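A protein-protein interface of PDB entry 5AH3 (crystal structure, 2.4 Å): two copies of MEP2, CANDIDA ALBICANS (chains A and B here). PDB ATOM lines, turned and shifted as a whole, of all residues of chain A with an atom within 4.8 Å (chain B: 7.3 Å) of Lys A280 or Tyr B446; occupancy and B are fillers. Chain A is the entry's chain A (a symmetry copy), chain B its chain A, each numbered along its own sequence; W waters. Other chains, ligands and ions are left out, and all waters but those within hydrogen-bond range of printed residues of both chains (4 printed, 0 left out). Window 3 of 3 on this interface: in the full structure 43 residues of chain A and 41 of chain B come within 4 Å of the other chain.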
ATOM      1  N   TYR A 217      21.079  20.928  36.272  1.00  0.00           N
ATOM      2  CA  TYR A 217      22.490  20.584  36.333  1.00  0.00           C
ATOM      3  C   TYR A 217      23.328  21.663  35.665  1.00  0.00           C
ATOM      4  O   TYR A 217      23.102  22.016  34.504  1.00  0.00           O
ATOM      5  CB  TYR A 217      22.756  19.223  35.661  1.00  0.00           C
ATOM      6  CG  TYR A 217      21.809  18.119  36.074  1.00  0.00           C
ATOM      7  CD1 TYR A 217      21.980  17.432  37.281  1.00  0.00           C
ATOM      8  CD2 TYR A 217      20.745  17.749  35.262  1.00  0.00           C
ATOM      9  CE1 TYR A 217      21.113  16.402  37.661  1.00  0.00           C
ATOM     10  CE2 TYR A 217      19.873  16.735  35.634  1.00  0.00           C
ATOM     11  CZ  TYR A 217      20.068  16.057  36.836  1.00  0.00           C
ATOM     12  OH  TYR A 217      19.201  15.045  37.209  1.00  0.00           O
ATOM     13  N   ASP A 273      16.495  11.125  33.409  1.00  0.00           N
ATOM     14  CA  ASP A 273      16.881  12.408  32.859  1.00  0.00           C
ATOM     15  C   ASP A 273      16.621  12.475  31.351  1.00  0.00           C
ATOM     16  O   ASP A 273      16.247  13.516  30.820  1.00  0.00           O
ATOM     17  CB  ASP A 273      18.358  12.682  33.152  1.00  0.00           C
ATOM     18  CG  ASP A 273      18.576  13.276  34.525  1.00  0.00           C
ATOM     19  OD1 ASP A 273      17.595  13.566  35.227  1.00  0.00           O
ATOM     20  OD2 ASP A 273      19.734  13.483  34.898  1.00  0.00           O
ATOM     21  N   TRP A 274      16.821  11.354  30.675  1.00  0.00           N
ATOM     22  CA  TRP A 274      16.577  11.255  29.250  1.00  0.00           C
ATOM     23  C   TRP A 274      15.094  11.497  28.920  1.00  0.00           C
ATOM     24  O   TRP A 274      14.767  12.227  27.980  1.00  0.00           O
ATOM     25  CB  TRP A 274      17.043   9.889  28.752  1.00  0.00           C
ATOM     26  CG  TRP A 274      16.901   9.686  27.293  1.00  0.00           C
ATOM     27  CD1 TRP A 274      17.811  10.006  26.323  1.00  0.00           C
ATOM     28  CD2 TRP A 274      15.787   9.097  26.620  1.00  0.00           C
ATOM     29  NE1 TRP A 274      17.325   9.656  25.087  1.00  0.00           N
ATOM     30  CE2 TRP A 274      16.082   9.098  25.242  1.00  0.00           C
ATOM     31  CE3 TRP A 274      14.563   8.572  27.049  1.00  0.00           C
ATOM     32  CZ2 TRP A 274      15.199   8.597  24.291  1.00  0.00           C
ATOM     33  CZ3 TRP A 274      13.688   8.072  26.104  1.00  0.00           C
ATOM     34  CH2 TRP A 274      14.010   8.090  24.741  1.00  0.00           C
ATOM     35  N   THR A 277      14.164  15.299  29.872  1.00  0.00           N
ATOM     36  CA  THR A 277      14.755  16.341  29.032  1.00  0.00           C
ATOM     37  C   THR A 277      14.367  16.216  27.558  1.00  0.00           C
ATOM     38  O   THR A 277      14.679  17.094  26.749  1.00  0.00           O
ATOM     39  CB  THR A 277      16.294  16.353  29.099  1.00  0.00           C
ATOM     40  OG1 THR A 277      16.814  15.074  28.713  1.00  0.00           O
ATOM     41  CG2 THR A 277      16.777  16.740  30.482  1.00  0.00           C
ATOM     42  N   GLY A 278      13.693  15.126  27.214  1.00  0.00           N
ATOM     43  CA  GLY A 278      13.326  14.881  25.835  1.00  0.00           C
ATOM     44  C   GLY A 278      14.505  14.420  24.996  1.00  0.00           C
ATOM     45  O   GLY A 278      14.653  14.846  23.849  1.00  0.00           O
ATOM     46  N   GLY A 279      15.364  13.575  25.568  1.00  0.00           N
ATOM     47  CA  GLY A 279      16.385  12.904  24.781  1.00  0.00           C
ATOM     48  C   GLY A 279      17.842  13.282  24.977  1.00  0.00           C
ATOM     49  O   GLY A 279      18.692  12.884  24.181  1.00  0.00           O
ATOM     50  N   LYS A 280      18.148  14.034  26.027  1.00  0.00           N
ATOM     51  CA  LYS A 280      19.542  14.371  26.340  1.00  0.00           C
ATOM     52  C   LYS A 280      20.186  13.297  27.216  1.00  0.00           C
ATOM     53  O   LYS A 280      19.502  12.639  27.994  1.00  0.00           O
ATOM     54  CB  LYS A 280      19.627  15.724  27.045  1.00  0.00           C
ATOM     55  CG  LYS A 280      19.061  16.902  26.242  1.00  0.00           C
ATOM     56  CD  LYS A 280      19.519  18.219  26.842  1.00  0.00           C
ATOM     57  CE  LYS A 280      18.888  19.419  26.142  1.00  0.00           C
ATOM     58  NZ  LYS A 280      17.424  19.521  26.410  1.00  0.00           N
ATOM     59  N   TRP A 281      21.496  13.119  27.086  1.00  0.00           N
ATOM     60  CA  TRP A 281      22.216  12.186  27.940  1.00  0.00           C
ATOM     61  C   TRP A 281      22.971  12.963  29.027  1.00  0.00           C
ATOM     62  O   TRP A 281      23.863  13.757  28.745  1.00  0.00           O
ATOM     63  CB  TRP A 281      23.171  11.308  27.118  1.00  0.00           C
ATOM     64  CG  TRP A 281      22.489  10.397  26.107  1.00  0.00           C
ATOM     65  CD1 TRP A 281      22.571  10.475  24.742  1.00  0.00           C
ATOM     66  CD2 TRP A 281      21.644   9.273  26.387  1.00  0.00           C
ATOM     67  NE1 TRP A 281      21.828   9.477  24.163  1.00  0.00           N
ATOM     68  CE2 TRP A 281      21.245   8.727  25.150  1.00  0.00           C
ATOM     69  CE3 TRP A 281      21.179   8.678  27.569  1.00  0.00           C
ATOM     70  CZ2 TRP A 281      20.408   7.613  25.057  1.00  0.00           C
ATOM     71  CZ3 TRP A 281      20.343   7.575  27.475  1.00  0.00           C
ATOM     72  CH2 TRP A 281      19.972   7.053  26.231  1.00  0.00           C
ATOM     73  N   SER A 282      22.598  12.719  30.277  1.00  0.00           N
ATOM     74  CA  SER A 282      23.071  13.504  31.410  1.00  0.00           C
ATOM     75  C   SER A 282      24.366  12.936  32.010  1.00  0.00           C
ATOM     76  O   SER A 282      24.374  11.823  32.549  1.00  0.00           O
ATOM     77  CB  SER A 282      21.958  13.567  32.464  1.00  0.00           C
ATOM     78  OG  SER A 282      22.338  14.299  33.607  1.00  0.00           O
ATOM     79  N   THR A 283      25.462  13.693  31.911  1.00  0.00           N
ATOM     80  CA  THR A 283      26.748  13.222  32.433  1.00  0.00           C
ATOM     81  C   THR A 283      26.802  13.299  33.957  1.00  0.00           C
ATOM     82  O   THR A 283      27.353  12.419  34.619  1.00  0.00           O
ATOM     83  CB  THR A 283      27.937  14.015  31.857  1.00  0.00           C
ATOM     84  OG1 THR A 283      27.607  15.403  31.801  1.00  0.00           O
ATOM     85  CG2 THR A 283      28.280  13.518  30.457  1.00  0.00           C
ATOM     86  N   ALA B  58      34.388  14.220  20.770  1.00  0.00           N
ATOM     87  CA  ALA B  58      33.200  14.806  21.382  1.00  0.00           C
ATOM     88  C   ALA B  58      32.813  14.077  22.688  1.00  0.00           C
ATOM     89  O   ALA B  58      32.338  14.696  23.635  1.00  0.00           O
ATOM     90  CB  ALA B  58      32.045  14.794  20.402  1.00  0.00           C
ATOM     91  N   ASP B 439      32.169  23.458  22.298  1.00  0.00           N
ATOM     92  CA  ASP B 439      31.793  22.618  23.432  1.00  0.00           C
ATOM     93  C   ASP B 439      32.854  22.587  24.533  1.00  0.00           C
ATOM     94  O   ASP B 439      34.034  22.387  24.256  1.00  0.00           O
ATOM     95  CB  ASP B 439      31.508  21.187  22.969  1.00  0.00           C
ATOM     96  CG  ASP B 439      30.938  20.328  24.085  1.00  0.00           C
ATOM     97  OD1 ASP B 439      29.975  20.773  24.744  1.00  0.00           O
ATOM     98  OD2 ASP B 439      31.459  19.219  24.314  1.00  0.00           O
ATOM     99  N   ASP B 440      32.409  22.787  25.770  1.00  0.00           N
ATOM    100  CA  ASP B 440      33.250  22.680  26.955  1.00  0.00           C
ATOM    101  C   ASP B 440      32.840  21.466  27.826  1.00  0.00           C
ATOM    102  O   ASP B 440      31.916  21.541  28.631  1.00  0.00           O
ATOM    103  CB  ASP B 440      33.166  23.979  27.755  1.00  0.00           C
ATOM    104  CG  ASP B 440      34.138  24.019  28.918  1.00  0.00           C
ATOM    105  OD1 ASP B 440      34.963  23.082  29.062  1.00  0.00           O
ATOM    106  OD2 ASP B 440      34.089  25.007  29.683  1.00  0.00           O
ATOM    107  N   PRO B 441      33.527  20.340  27.647  1.00  0.00           N
ATOM    108  CA  PRO B 441      33.314  19.090  28.388  1.00  0.00           C
ATOM    109  C   PRO B 441      33.380  19.235  29.920  1.00  0.00           C
ATOM    110  O   PRO B 441      32.704  18.482  30.627  1.00  0.00           O
ATOM    111  CB  PRO B 441      34.442  18.210  27.871  1.00  0.00           C
ATOM    112  CG  PRO B 441      34.614  18.661  26.465  1.00  0.00           C
ATOM    113  CD  PRO B 441      34.488  20.159  26.546  1.00  0.00           C
ATOM    114  N   THR B 443      32.139  21.686  31.701  1.00  0.00           N
ATOM    115  CA  THR B 443      31.005  22.369  32.311  1.00  0.00           C
ATOM    116  C   THR B 443      29.686  21.991  31.659  1.00  0.00           C
ATOM    117  O   THR B 443      28.620  22.333  32.171  1.00  0.00           O
ATOM    118  CB  THR B 443      31.171  23.915  32.247  1.00  0.00           C
ATOM    119  OG1 THR B 443      31.171  24.340  30.882  1.00  0.00           O
ATOM    120  CG2 THR B 443      32.474  24.344  32.894  1.00  0.00           C
ATOM    121  N   ASN B 444      29.754  21.297  30.526  1.00  0.00           N
ATOM    122  CA  ASN B 444      28.544  20.875  29.827  1.00  0.00           C
ATOM    123  C   ASN B 444      27.915  19.686  30.551  1.00  0.00           C
ATOM    124  O   ASN B 444      28.526  18.629  30.660  1.00  0.00           O
ATOM    125  CB  ASN B 444      28.849  20.518  28.367  1.00  0.00           C
ATOM    126  CG  ASN B 444      27.594  20.326  27.534  1.00  0.00           C
ATOM    127  OD1 ASN B 444      26.502  20.229  28.064  1.00  0.00           O
ATOM    128  ND2 ASN B 444      27.752  20.268  26.221  1.00  0.00           N
ATOM    129  N   PRO B 445      26.681  19.861  31.041  1.00  0.00           N
ATOM    130  CA  PRO B 445      25.967  18.821  31.783  1.00  0.00           C
ATOM    131  C   PRO B 445      25.506  17.648  30.908  1.00  0.00           C
ATOM    132  O   PRO B 445      25.096  16.624  31.454  1.00  0.00           O
ATOM    133  CB  PRO B 445      24.751  19.561  32.356  1.00  0.00           C
ATOM    134  CG  PRO B 445      24.969  21.017  32.049  1.00  0.00           C
ATOM    135  CD  PRO B 445      25.894  21.098  30.914  1.00  0.00           C
ATOM    136  N   TYR B 446      25.575  17.794  29.587  1.00  0.00           N
ATOM    137  CA  TYR B 446      25.061  16.769  28.687  1.00  0.00           C
ATOM    138  C   TYR B 446      26.104  16.302  27.679  1.00  0.00           C
ATOM    139  O   TYR B 446      27.014  17.050  27.318  1.00  0.00           O
ATOM    140  CB  TYR B 446      23.813  17.286  27.963  1.00  0.00           C
ATOM    141  CG  TYR B 446      22.741  17.732  28.926  1.00  0.00           C
ATOM    142  CD1 TYR B 446      22.205  16.847  29.846  1.00  0.00           C
ATOM    143  CD2 TYR B 446      22.273  19.035  28.928  1.00  0.00           C
ATOM    144  CE1 TYR B 446      21.234  17.242  30.748  1.00  0.00           C
ATOM    145  CE2 TYR B 446      21.291  19.442  29.826  1.00  0.00           C
ATOM    146  CZ  TYR B 446      20.780  18.540  30.737  1.00  0.00           C
ATOM    147  OH  TYR B 446      19.810  18.921  31.640  1.00  0.00           O
ATOM    148  N   VAL B 447      25.988  15.044  27.257  1.00  0.00           N
ATOM    149  CA  VAL B 447      26.844  14.515  26.202  1.00  0.00           C
ATOM    150  C   VAL B 447      26.602  15.299  24.911  1.00  0.00           C
ATOM    151  O   VAL B 447      25.455  15.487  24.515  1.00  0.00           O
ATOM    152  CB  VAL B 447      26.580  13.018  25.944  1.00  0.00           C
ATOM    153  CG1 VAL B 447      27.262  12.576  24.669  1.00  0.00           C
ATOM    154  CG2 VAL B 447      27.041  12.166  27.129  1.00  0.00           C
ATOM    155  N   LEU B 448      27.674  15.763  24.270  1.00  0.00           N
ATOM    156  CA  LEU B 448      27.571  16.409  22.962  1.00  0.00           C
ATOM    157  C   LEU B 448      27.261  15.375  21.881  1.00  0.00           C
ATOM    158  O   LEU B 448      28.172  14.803  21.275  1.00  0.00           O
ATOM    159  CB  LEU B 448      28.864  17.154  22.613  1.00  0.00           C
ATOM    160  CG  LEU B 448      28.825  18.108  21.409  1.00  0.00           C
ATOM    161  CD1 LEU B 448      28.106  19.384  21.785  1.00  0.00           C
ATOM    162  CD2 LEU B 448      30.220  18.428  20.889  1.00  0.00           C
ATOM    163  N   GLU B 449      25.977  15.136  21.644  1.00  0.00           N
ATOM    164  CA  GLU B 449      25.555  14.151  20.663  1.00  0.00           C
ATOM    165  C   GLU B 449      25.883  14.600  19.250  1.00  0.00           C
ATOM    166  O   GLU B 449      25.695  15.769  18.903  1.00  0.00           O
ATOM    167  CB  GLU B 449      24.058  13.873  20.783  1.00  0.00           C
ATOM    168  CG  GLU B 449      23.712  12.773  21.783  1.00  0.00           C
ATOM    169  CD  GLU B 449      24.178  11.397  21.333  1.00  0.00           C
ATOM    170  OE1 GLU B 449      23.593  10.869  20.370  1.00  0.00           O
ATOM    171  OE2 GLU B 449      25.128  10.851  21.932  1.00  0.00           O
HETATM  172  O   HOH W   1      29.946  16.565  29.932  1.00  0.00           O
HETATM  173  O   HOH W   2      23.032  14.816  25.131  1.00  0.00           O
HETATM  174  O   HOH W   3      23.910  16.387  33.548  1.00  0.00           O
HETATM  175  O   HOH W   4      20.548  21.101  33.380  1.00  0.00           O
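No position is printed for both chains. Of the 13 pairs that touch across the chains among the printed residues, none has its exchanged pair printed and touching as well.
Hydrophobic or aromatic side chains of chain A within 4 Å of the printed part of chain B: Tyr A217 and Trp A281. Of the 11 printed residues of chain B, 5 touch a printed residue of chain A. Printed residues of chain B that touch a printed residue of chain A: Asn B444, Pro B445, Tyr B446, Val B447 and Glu B449. Along chain B the printed residues that touch a printed residue of chain A span positions 444 to 449. Among the printed residues, no Asp or Glu carboxylate lies within 4 Å of a Lys or Arg side-chain nitrogen of the other chain.
Water W3 lies within hydrogen-bond range of O of Pro B445 and OG of Ser A282. Water W2 bridges the backbone carbonyl oxygen (O) of Val B447 and the backbone NH (N) of Trp A281. Water W1 lies within hydrogen-bond range of O of Asn B444 (2.6 Å), OG1 of Thr A283 (3.2 Å) and O of Pro B441 (3.4 Å). Water W4 lies within hydrogen-bond range of the side-chain hydroxyl of Tyr B446 and the backbone carbonyl oxygen of Tyr A217.
The side-chain hydroxyl (OG1) of Thr A283 lies within hydrogen-bond range of the backbone carbonyl oxygen (O) of Pro B445, 2.8 Å away. The backbone carbonyl oxygen (O) of Trp A281 sits at hydrogen-bond distance from the backbone NH (N) of Val B447 (2.9 Å).
No residue of chain B comes within 4 Å of Gly A279. Of chain B, only Tyr B446 (3.5 Å) comes within 4 Å of Lys A280. Of the printed residues of chain B, Trp A281 touches Tyr B446 (3.2 Å), Val B447 (2.9 Å) and Glu B449 (3.8 Å). Of the printed residues of chain B, Thr A283 touches Asn B444 (3.5 Å), Pro B445 (2.8 Å), Tyr B446 (3.8 Å) and Val B447 (3.8 Å). Asp B440 touches none of the printed residues of chain A. Of the printed residues of chain A, Asn B444 touches Thr A283 (3.5 Å). Printed residues of chain A within 4 Å of Val B447: Trp A281 and Thr A283. The nearest residue of chain B that does not touch Lys A280 is Val B447 (6.1 Å). The nearest printed residue of chain A that does not touch Tyr B446 is Asp A273 (5.8 Å).
OD1 of Asp B439 lies within hydrogen-bond range of ND2 of Asn B444 (2.7 Å). OG of Ser A282 sits at hydrogen-bond distance from OD2 of Asp A273. The side-chain amide oxygen of Asn B444 is in hydrogen-bond range of the backbone NH of Tyr B446 (3.0 Å). The backbone carbonyl oxygen (O) of Asp A273 is in hydrogen-bond range of the side-chain hydroxyl (OG1) of Thr A277 (2.7 Å). OD2 of Asp A273 lies within hydrogen-bond range of OH of Tyr A217 (2.8 Å). The side-chain hydroxyl of Thr A277 sits at hydrogen-bond distance from the backbone NH of Lys A280, 3.2 Å away.
O of Tyr A217 touches CG of Pro B445, at 3.2 Å. Tyr A217 touches Tyr B446. Tyr B446 touches Thr A277 (OH to CG2, 3.9 Å). CD of Lys A280 touches CD2 of Tyr B446, at 3.5 Å. Trp A281 touches Tyr B446. Ser A282 touches Pro B445. CA of Ser A282 touches CD1 of Tyr B446, 3.8 Å away. Asn B444 touches Thr A283. N of Tyr B446 touches OG1 of Thr A283, at 3.8 Å. CG2 of Val B447 touches CG2 of Thr A283 (3.8 Å).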
